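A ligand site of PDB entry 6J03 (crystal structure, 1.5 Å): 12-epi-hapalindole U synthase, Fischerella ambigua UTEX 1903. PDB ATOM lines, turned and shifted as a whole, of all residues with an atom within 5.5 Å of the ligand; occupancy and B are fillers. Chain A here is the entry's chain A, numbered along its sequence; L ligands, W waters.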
ATOM      1  N   ASP A  21     -33.682   5.570   8.688  1.00  0.00           N
ATOM      2  CA  ASP A  21     -32.731   4.812   7.849  1.00  0.00           C
ATOM      3  C   ASP A  21     -31.556   5.704   7.429  1.00  0.00           C
ATOM      4  O   ASP A  21     -30.626   5.169   6.823  1.00  0.00           O
ATOM      5  CB  ASP A  21     -33.397   4.107   6.673  1.00  0.00           C
ATOM      6  CG  ASP A  21     -34.273   2.938   7.084  1.00  0.00           C
ATOM      7  OD1 ASP A  21     -34.010   2.361   8.164  1.00  0.00           O
ATOM      8  OD2 ASP A  21     -35.219   2.621   6.328  1.00  0.00           O
ATOM      9  N   ASP A  22     -31.477   6.956   7.889  1.00  0.00           N
ATOM     10  CA  ASP A  22     -30.219   7.696   7.688  1.00  0.00           C
ATOM     11  C   ASP A  22     -29.188   7.191   8.711  1.00  0.00           C
ATOM     12  O   ASP A  22     -29.537   6.502   9.698  1.00  0.00           O
ATOM     13  CB  ASP A  22     -30.347   9.203   7.750  1.00  0.00           C
ATOM     14  CG  ASP A  22     -29.225   9.942   7.006  1.00  0.00           C
ATOM     15  OD1 ASP A  22     -28.370   9.249   6.285  1.00  0.00           O
ATOM     16  OD2 ASP A  22     -29.211  11.206   7.101  1.00  0.00           O
ATOM     17  N   TYR A  23     -27.932   7.461   8.423  1.00  0.00           N
ATOM     18  CA  TYR A  23     -26.805   6.964   9.220  1.00  0.00           C
ATOM     19  C   TYR A  23     -25.624   7.930   9.124  1.00  0.00           C
ATOM     20  O   TYR A  23     -25.512   8.684   8.133  1.00  0.00           O
ATOM     21  CB  TYR A  23     -26.436   5.544   8.789  1.00  0.00           C
ATOM     22  CG  TYR A  23     -25.914   5.395   7.374  1.00  0.00           C
ATOM     23  CD1 TYR A  23     -26.781   5.279   6.316  1.00  0.00           C
ATOM     24  CD2 TYR A  23     -24.554   5.251   7.133  1.00  0.00           C
ATOM     25  CE1 TYR A  23     -26.311   5.066   5.027  1.00  0.00           C
ATOM     26  CE2 TYR A  23     -24.072   4.971   5.854  1.00  0.00           C
ATOM     27  CZ  TYR A  23     -24.955   4.901   4.800  1.00  0.00           C
ATOM     28  OH  TYR A  23     -24.475   4.659   3.539  1.00  0.00           O
ATOM     29  N   ILE A  25     -21.215   7.980   9.406  1.00  0.00           N
ATOM     30  CA  ILE A  25     -20.068   7.091   9.081  1.00  0.00           C
ATOM     31  C   ILE A  25     -18.860   7.486   9.915  1.00  0.00           C
ATOM     32  O   ILE A  25     -17.753   7.024   9.568  1.00  0.00           O
ATOM     33  CB  ILE A  25     -19.760   7.135   7.578  1.00  0.00           C
ATOM     34  CG1 ILE A  25     -19.394   8.543   7.098  1.00  0.00           C
ATOM     35  CG2 ILE A  25     -20.906   6.540   6.809  1.00  0.00           C
ATOM     36  CD1 ILE A  25     -18.897   8.604   5.662  1.00  0.00           C
ATOM     37  N   THR A  45     -15.795   6.997   4.275  1.00  0.00           N
ATOM     38  CA  THR A  45     -16.742   7.083   3.150  1.00  0.00           C
ATOM     39  C   THR A  45     -17.803   6.010   3.343  1.00  0.00           C
ATOM     40  O   THR A  45     -17.552   5.003   3.987  1.00  0.00           O
ATOM     41  CB  THR A  45     -16.079   6.921   1.778  1.00  0.00           C
ATOM     42  OG1 THR A  45     -15.492   5.620   1.661  1.00  0.00           O
ATOM     43  CG2 THR A  45     -15.039   7.992   1.501  1.00  0.00           C
ATOM     44  N   THR A  46     -18.952   6.221   2.753  1.00  0.00           N
ATOM     45  CA  THR A  46     -19.944   5.150   2.632  1.00  0.00           C
ATOM     46  C   THR A  46     -19.366   4.032   1.765  1.00  0.00           C
ATOM     47  O   THR A  46     -18.442   4.278   0.982  1.00  0.00           O
ATOM     48  CB  THR A  46     -21.269   5.676   2.085  1.00  0.00           C
ATOM     49  OG1 THR A  46     -21.028   6.141   0.753  1.00  0.00           O
ATOM     50  CG2 THR A  46     -21.885   6.743   2.968  1.00  0.00           C
ATOM     51  N   TRP A  47     -19.848   2.815   1.991  1.00  0.00           N
ATOM     52  CA  TRP A  47     -19.543   1.620   1.157  1.00  0.00           C
ATOM     53  C   TRP A  47     -18.117   1.111   1.387  1.00  0.00           C
ATOM     54  O   TRP A  47     -17.718   0.208   0.673  1.00  0.00           O
ATOM     55  CB  TRP A  47     -19.794   1.909  -0.326  1.00  0.00           C
ATOM     56  CG  TRP A  47     -21.245   2.081  -0.622  1.00  0.00           C
ATOM     57  CD1 TRP A  47     -22.024   3.195  -0.408  1.00  0.00           C
ATOM     58  CD2 TRP A  47     -22.154   1.022  -0.954  1.00  0.00           C
ATOM     59  NE1 TRP A  47     -23.308   2.929  -0.785  1.00  0.00           N
ATOM     60  CE2 TRP A  47     -23.431   1.593  -1.055  1.00  0.00           C
ATOM     61  CE3 TRP A  47     -21.996  -0.362  -1.173  1.00  0.00           C
ATOM     62  CZ2 TRP A  47     -24.553   0.831  -1.399  1.00  0.00           C
ATOM     63  CZ3 TRP A  47     -23.103  -1.109  -1.467  1.00  0.00           C
ATOM     64  CH2 TRP A  47     -24.367  -0.512  -1.601  1.00  0.00           C
ATOM     65  N   THR A  48     -17.428   1.638   2.375  1.00  0.00           N
ATOM     66  CA  THR A  48     -16.137   1.120   2.864  1.00  0.00           C
ATOM     67  C   THR A  48     -16.264   0.877   4.373  1.00  0.00           C
ATOM     68  O   THR A  48     -17.278   1.237   4.966  1.00  0.00           O
ATOM     69  CB  THR A  48     -14.975   2.070   2.542  1.00  0.00           C
ATOM     70  OG1 THR A  48     -15.231   3.305   3.197  1.00  0.00           O
ATOM     71  CG2 THR A  48     -14.817   2.310   1.061  1.00  0.00           C
ATOM     72  N   ASN A  50     -16.607   1.129   8.097  1.00  0.00           N
ATOM     73  CA  ASN A  50     -16.966   2.336   8.855  1.00  0.00           C
ATOM     74  C   ASN A  50     -17.807   1.921  10.048  1.00  0.00           C
ATOM     75  O   ASN A  50     -18.119   0.747  10.238  1.00  0.00           O
ATOM     76  CB  ASN A  50     -17.628   3.393   7.954  1.00  0.00           C
ATOM     77  CG  ASN A  50     -18.824   2.884   7.179  1.00  0.00           C
ATOM     78  OD1 ASN A  50     -19.525   1.971   7.626  1.00  0.00           O
ATOM     79  ND2 ASN A  50     -19.101   3.510   6.024  1.00  0.00           N
ATOM     80  N   VAL A  53     -23.871   5.754  13.693  1.00  0.00           N
ATOM     81  CA  VAL A  53     -25.217   5.497  14.234  1.00  0.00           C
ATOM     82  C   VAL A  53     -26.194   5.392  13.066  1.00  0.00           C
ATOM     83  O   VAL A  53     -25.913   5.906  11.972  1.00  0.00           O
ATOM     84  CB  VAL A  53     -25.641   6.569  15.242  1.00  0.00           C
ATOM     85  CG1 VAL A  53     -24.573   6.741  16.316  1.00  0.00           C
ATOM     86  CG2 VAL A  53     -26.002   7.894  14.590  1.00  0.00           C
ATOM     87  N   GLY A  54     -27.278   4.670  13.306  1.00  0.00           N
ATOM     88  CA  GLY A  54     -28.382   4.559  12.336  1.00  0.00           C
ATOM     89  C   GLY A  54     -29.723   4.717  13.018  1.00  0.00           C
ATOM     90  O   GLY A  54     -29.917   4.204  14.119  1.00  0.00           O
ATOM     91  N   TYR A  55     -30.616   5.480  12.386  1.00  0.00           N
ATOM     92  CA  TYR A  55     -31.957   5.774  12.935  1.00  0.00           C
ATOM     93  C   TYR A  55     -32.904   4.645  12.530  1.00  0.00           C
ATOM     94  O   TYR A  55     -33.303   4.515  11.358  1.00  0.00           O
ATOM     95  CB  TYR A  55     -32.392   7.147  12.437  1.00  0.00           C
ATOM     96  CG  TYR A  55     -33.767   7.585  12.891  1.00  0.00           C
ATOM     97  CD1 TYR A  55     -34.432   6.984  13.937  1.00  0.00           C
ATOM     98  CD2 TYR A  55     -34.325   8.724  12.344  1.00  0.00           C
ATOM     99  CE1 TYR A  55     -35.697   7.401  14.328  1.00  0.00           C
ATOM    100  CE2 TYR A  55     -35.567   9.172  12.723  1.00  0.00           C
ATOM    101  CZ  TYR A  55     -36.276   8.503  13.704  1.00  0.00           C
ATOM    102  OH  TYR A  55     -37.515   8.962  14.017  1.00  0.00           O
ATOM    103  N   VAL A  56     -33.238   3.802  13.493  1.00  0.00           N
ATOM    104  CA  VAL A  56     -34.173   2.653  13.288  1.00  0.00           C
ATOM    105  C   VAL A  56     -35.524   3.037  13.879  1.00  0.00           C
ATOM    106  O   VAL A  56     -35.763   2.758  15.072  1.00  0.00           O
ATOM    107  CB  VAL A  56     -33.620   1.345  13.863  1.00  0.00           C
ATOM    108  CG1 VAL A  56     -34.569   0.193  13.566  1.00  0.00           C
ATOM    109  CG2 VAL A  56     -32.219   1.063  13.323  1.00  0.00           C
ATOM    110  N   TYR A  63     -35.493  -3.358   9.075  1.00  0.00           N
ATOM    111  CA  TYR A  63     -35.652  -4.060  10.361  1.00  0.00           C
ATOM    112  C   TYR A  63     -37.109  -4.484  10.546  1.00  0.00           C
ATOM    113  O   TYR A  63     -38.032  -3.842   9.977  1.00  0.00           O
ATOM    114  CB  TYR A  63     -35.206  -3.178  11.528  1.00  0.00           C
ATOM    115  CG  TYR A  63     -33.746  -2.805  11.463  1.00  0.00           C
ATOM    116  CD1 TYR A  63     -33.312  -1.715  10.727  1.00  0.00           C
ATOM    117  CD2 TYR A  63     -32.789  -3.548  12.132  1.00  0.00           C
ATOM    118  CE1 TYR A  63     -31.974  -1.382  10.644  1.00  0.00           C
ATOM    119  CE2 TYR A  63     -31.441  -3.224  12.047  1.00  0.00           C
ATOM    120  CZ  TYR A  63     -31.030  -2.130  11.317  1.00  0.00           C
ATOM    121  OH  TYR A  63     -29.724  -1.762  11.254  1.00  0.00           O
ATOM    122  N   ILE A  73     -29.374   2.915  16.640  1.00  0.00           N
ATOM    123  CA  ILE A  73     -28.413   1.846  16.975  1.00  0.00           C
ATOM    124  C   ILE A  73     -27.014   2.333  16.596  1.00  0.00           C
ATOM    125  O   ILE A  73     -26.885   3.349  15.864  1.00  0.00           O
ATOM    126  CB  ILE A  73     -28.826   0.520  16.306  1.00  0.00           C
ATOM    127  CG1 ILE A  73     -28.832   0.568  14.773  1.00  0.00           C
ATOM    128  CG2 ILE A  73     -30.183   0.091  16.817  1.00  0.00           C
ATOM    129  CD1 ILE A  73     -27.461   0.629  14.116  1.00  0.00           C
ATOM    130  N   TYR A  75     -23.572   0.901  14.630  1.00  0.00           N
ATOM    131  CA  TYR A  75     -23.233  -0.205  13.702  1.00  0.00           C
ATOM    132  C   TYR A  75     -21.740  -0.200  13.415  1.00  0.00           C
ATOM    133  O   TYR A  75     -21.070   0.847  13.490  1.00  0.00           O
ATOM    134  CB  TYR A  75     -24.035  -0.100  12.405  1.00  0.00           C
ATOM    135  CG  TYR A  75     -23.524   0.968  11.473  1.00  0.00           C
ATOM    136  CD1 TYR A  75     -22.455   0.686  10.633  1.00  0.00           C
ATOM    137  CD2 TYR A  75     -23.977   2.274  11.545  1.00  0.00           C
ATOM    138  CE1 TYR A  75     -21.846   1.676   9.880  1.00  0.00           C
ATOM    139  CE2 TYR A  75     -23.400   3.276  10.776  1.00  0.00           C
ATOM    140  CZ  TYR A  75     -22.308   2.978   9.972  1.00  0.00           C
ATOM    141  OH  TYR A  75     -21.703   3.940   9.221  1.00  0.00           O
ATOM    142  N   TYR A  77     -19.594  -1.734  10.097  1.00  0.00           N
ATOM    143  CA  TYR A  77     -19.643  -2.378   8.776  1.00  0.00           C
ATOM    144  C   TYR A  77     -18.223  -2.573   8.289  1.00  0.00           C
ATOM    145  O   TYR A  77     -17.450  -1.612   8.269  1.00  0.00           O
ATOM    146  CB  TYR A  77     -20.452  -1.539   7.789  1.00  0.00           C
ATOM    147  CG  TYR A  77     -20.301  -2.018   6.369  1.00  0.00           C
ATOM    148  CD1 TYR A  77     -20.726  -3.275   6.011  1.00  0.00           C
ATOM    149  CD2 TYR A  77     -19.645  -1.253   5.418  1.00  0.00           C
ATOM    150  CE1 TYR A  77     -20.489  -3.782   4.737  1.00  0.00           C
ATOM    151  CE2 TYR A  77     -19.438  -1.726   4.138  1.00  0.00           C
ATOM    152  CZ  TYR A  77     -19.808  -3.027   3.809  1.00  0.00           C
ATOM    153  OH  TYR A  77     -19.577  -3.523   2.554  1.00  0.00           O
ATOM    154  N   LEU A 112     -28.967  -5.645   9.965  1.00  0.00           N
ATOM    155  CA  LEU A 112     -29.858  -5.294   8.852  1.00  0.00           C
ATOM    156  C   LEU A 112     -30.545  -6.529   8.290  1.00  0.00           C
ATOM    157  O   LEU A 112     -29.948  -7.631   8.304  1.00  0.00           O
ATOM    158  CB  LEU A 112     -29.031  -4.621   7.759  1.00  0.00           C
ATOM    159  CG  LEU A 112     -28.578  -3.198   8.083  1.00  0.00           C
ATOM    160  CD1 LEU A 112     -27.407  -2.804   7.179  1.00  0.00           C
ATOM    161  CD2 LEU A 112     -29.733  -2.224   7.946  1.00  0.00           C
ATOM    162  N   PHE A 116     -29.767  -3.766  -0.474  1.00  0.00           N
ATOM    163  CA  PHE A 116     -29.688  -2.319  -0.795  1.00  0.00           C
ATOM    164  C   PHE A 116     -28.794  -2.158  -2.015  1.00  0.00           C
ATOM    165  O   PHE A 116     -27.590  -2.411  -1.931  1.00  0.00           O
ATOM    166  CB  PHE A 116     -29.167  -1.512   0.396  1.00  0.00           C
ATOM    167  CG  PHE A 116     -29.160  -0.037   0.139  1.00  0.00           C
ATOM    168  CD1 PHE A 116     -30.357   0.644   0.035  1.00  0.00           C
ATOM    169  CD2 PHE A 116     -27.977   0.668  -0.012  1.00  0.00           C
ATOM    170  CE1 PHE A 116     -30.357   2.007  -0.207  1.00  0.00           C
ATOM    171  CE2 PHE A 116     -27.992   2.035  -0.214  1.00  0.00           C
ATOM    172  CZ  PHE A 116     -29.189   2.704  -0.277  1.00  0.00           C
ATOM    173  N   LEU A 119     -26.448  -4.982  -2.906  1.00  0.00           N
ATOM    174  CA  LEU A 119     -25.705  -5.611  -1.788  1.00  0.00           C
ATOM    175  C   LEU A 119     -26.705  -6.302  -0.855  1.00  0.00           C
ATOM    176  O   LEU A 119     -27.596  -5.634  -0.321  1.00  0.00           O
ATOM    177  CB  LEU A 119     -24.885  -4.564  -1.024  1.00  0.00           C
ATOM    178  CG  LEU A 119     -24.009  -5.134   0.090  1.00  0.00           C
ATOM    179  CD1 LEU A 119     -22.890  -5.990  -0.479  1.00  0.00           C
ATOM    180  CD2 LEU A 119     -23.442  -4.043   0.975  1.00  0.00           C
ATOM    181  N   PHE A 121     -28.073  -8.126   2.480  1.00  0.00           N
ATOM    182  CA  PHE A 121     -27.873  -8.092   3.952  1.00  0.00           C
ATOM    183  C   PHE A 121     -28.095  -9.473   4.552  1.00  0.00           C
ATOM    184  O   PHE A 121     -28.019  -9.592   5.759  1.00  0.00           O
ATOM    185  CB  PHE A 121     -28.751  -7.026   4.596  1.00  0.00           C
ATOM    186  CG  PHE A 121     -28.468  -5.627   4.112  1.00  0.00           C
ATOM    187  CD1 PHE A 121     -27.187  -5.234   3.769  1.00  0.00           C
ATOM    188  CD2 PHE A 121     -29.485  -4.695   3.996  1.00  0.00           C
ATOM    189  CE1 PHE A 121     -26.922  -3.935   3.369  1.00  0.00           C
ATOM    190  CE2 PHE A 121     -29.219  -3.396   3.595  1.00  0.00           C
ATOM    191  CZ  PHE A 121     -27.935  -3.015   3.311  1.00  0.00           C
ATOM    192  N   PHE A 184     -23.371 -11.180   5.035  1.00  0.00           N
ATOM    193  CA  PHE A 184     -23.120  -9.753   5.117  1.00  0.00           C
ATOM    194  C   PHE A 184     -22.405  -9.371   6.422  1.00  0.00           C
ATOM    195  O   PHE A 184     -22.850  -9.774   7.501  1.00  0.00           O
ATOM    196  CB  PHE A 184     -24.470  -9.034   5.020  1.00  0.00           C
ATOM    197  CG  PHE A 184     -24.417  -7.545   5.281  1.00  0.00           C
ATOM    198  CD1 PHE A 184     -23.775  -6.695   4.409  1.00  0.00           C
ATOM    199  CD2 PHE A 184     -24.994  -7.015   6.418  1.00  0.00           C
ATOM    200  CE1 PHE A 184     -23.701  -5.338   4.672  1.00  0.00           C
ATOM    201  CE2 PHE A 184     -24.948  -5.654   6.670  1.00  0.00           C
ATOM    202  CZ  PHE A 184     -24.284  -4.814   5.805  1.00  0.00           C
ATOM    203  N   GLY A 186     -22.006  -6.475   8.265  1.00  0.00           N
ATOM    204  CA  GLY A 186     -22.405  -5.370   9.141  1.00  0.00           C
ATOM    205  C   GLY A 186     -23.103  -5.906  10.373  1.00  0.00           C
ATOM    206  O   GLY A 186     -23.716  -6.962  10.295  1.00  0.00           O
ATOM    207  N   ASP A 188     -25.020  -4.565  14.363  1.00  0.00           N
ATOM    208  CA  ASP A 188     -25.576  -3.461  15.171  1.00  0.00           C
ATOM    209  C   ASP A 188     -25.507  -3.779  16.663  1.00  0.00           C
ATOM    210  O   ASP A 188     -25.708  -4.938  17.039  1.00  0.00           O
ATOM    211  CB  ASP A 188     -27.031  -3.206  14.803  1.00  0.00           C
ATOM    212  CG  ASP A 188     -27.301  -2.913  13.343  1.00  0.00           C
ATOM    213  OD1 ASP A 188     -26.379  -2.520  12.624  1.00  0.00           O
ATOM    214  OD2 ASP A 188     -28.494  -3.020  12.988  1.00  0.00           O
HETATM  215  N1  LIG L   1     -23.771  -0.089   4.672  1.00  0.00           N
HETATM  216  C1  LIG L   1     -23.332   1.112   4.159  1.00  0.00           C
HETATM  217  C2  LIG L   1     -22.927   0.770   2.693  1.00  0.00           C
HETATM  218  C3  LIG L   1     -23.993  -0.330   2.353  1.00  0.00           C
HETATM  219  C4  LIG L   1     -24.152  -1.094   3.545  1.00  0.00           C
HETATM  220  C5  LIG L   1     -22.135   1.763   4.909  1.00  0.00           C
HETATM  221  O1  LIG L   1     -21.290   2.414   4.383  1.00  0.00           O
HETATM  222  N2  LIG L   1     -22.110   1.452   6.269  1.00  0.00           N
HETATM  223  C6  LIG L   1     -23.182   0.719   6.881  1.00  0.00           C
HETATM  224  C7  LIG L   1     -23.703  -0.413   6.057  1.00  0.00           C
HETATM  225  O2  LIG L   1     -24.034  -1.487   6.453  1.00  0.00           O
HETATM  226  C8  LIG L   1     -24.360   1.696   7.284  1.00  0.00           C
HETATM  227  C9  LIG L   1     -25.445   0.956   8.114  1.00  0.00           C
HETATM  228  C10 LIG L   1     -26.496   1.973   8.551  1.00  0.00           C
HETATM  229  N3  LIG L   1     -27.471   1.308   9.382  1.00  0.00           N
HETATM  230  C11 LIG L   1     -28.766   1.816   9.638  1.00  0.00           C
HETATM  231  N4  LIG L   1     -29.477   1.007  10.549  1.00  0.00           N
HETATM  232  N5  LIG L   1     -29.249   2.917   9.150  1.00  0.00           N
HETATM  233  O   HOH W   1     -24.392  -2.457   9.111  1.00  0.00           O
HETATM  234  O   HOH W   2     -29.632   2.005   5.858  1.00  0.00           O
HETATM  235  O   HOH W   3     -26.716  -1.145  10.437  1.00  0.00           O
HETATM  236  O   HOH W   4     -31.971   2.407   9.966  1.00  0.00           O
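OH of Tyr 63 is in hydrogen-bond range of OD2 of Asp 188 (2.5 Å). OH of Tyr 75 sits close to OD1 of Asn 50 (3.3 Å). The backbone carbonyl oxygen (O) of Tyr 77 lies within hydrogen-bond range of the backbone NH (N) of Asn 50, 2.9 Å away. The backbone carbonyl oxygen (O) of Thr 48 sits at hydrogen-bond distance from the side-chain amide nitrogen (ND2) of Asn 50. The side-chain amide nitrogen (ND2) of Asn 50 lies within hydrogen-bond range of the backbone carbonyl oxygen (O) of Thr 45 (3.0 Å). The backbone carbonyl oxygen (O) of Tyr 55 sits at hydrogen-bond distance from the backbone NH (N) of Asp 21. The backbone NH (N) of Tyr 55 is in hydrogen-bond range of the backbone carbonyl oxygen (O) of Asp 22 (3.1 Å). N of Ile 73 lies within hydrogen-bond range of O of Gly 54, 2.9 Å away.
Merely in contact with the ligand: Asp 21 (3.5 Å), Asp 22 (3.6 Å), Tyr 23 (3.6 Å), Thr 46 (3.5 Å), Gly 54 (3.7 Å), Val 56 (3.9 Å), Tyr 75 (3.4 Å), Tyr 77 (3.7 Å), Leu 112 (3.7 Å), Leu 119 (3.98 Å), Phe 121 (3.97 Å) and Phe 184 (3.4 Å). Hydrophobic or aromatic side chains within 4 Å of the ligand: Tyr 23, Trp 47, Val 56, Tyr 63, Tyr 75, Tyr 77, Leu 112, Leu 119, Phe 121 and Phe 184. Within 4 Å of the ligand: Asp 21, Asp 22, Tyr 23, Thr 46, Trp 47, Asn 50, Gly 54, Val 56, Tyr 63, Tyr 75, Tyr 77, Leu 112, Leu 119, Phe 121 and Phe 184. The nearest printed residue that does not touch the ligand is Ile 73 (4.1 Å).
Water W3 lies within hydrogen-bond range of the side-chain carboxylate of Asp 188 (2.6 Å), a nitrogen (N3) of the ligand (2.8 Å) and the side-chain hydroxyl of Tyr 63 (3.2 Å). Water W4 lies within hydrogen-bond range of the side-chain carboxylate of Asp 21 (2.7 Å), the backbone carbonyl oxygen of Tyr 55 (2.9 Å) and a nitrogen (N5) of the ligand (2.9 Å). Water W2 bridges a nitrogen (N5) of the ligand (3.4 Å) and the backbone carbonyl oxygen of Asp 21 (3.5 Å).
The backbone NH (N) of Trp 47 lies within hydrogen-bond range of an oxygen (O1) of the ligand (2.8 Å). A nitrogen (N4) of the ligand lies within hydrogen-bond range of the side-chain hydroxyl of Tyr 63 (2.9 Å). ND2 of Asn 50 sits at hydrogen-bond distance from O1 of the ligand, 2.9 Å away.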
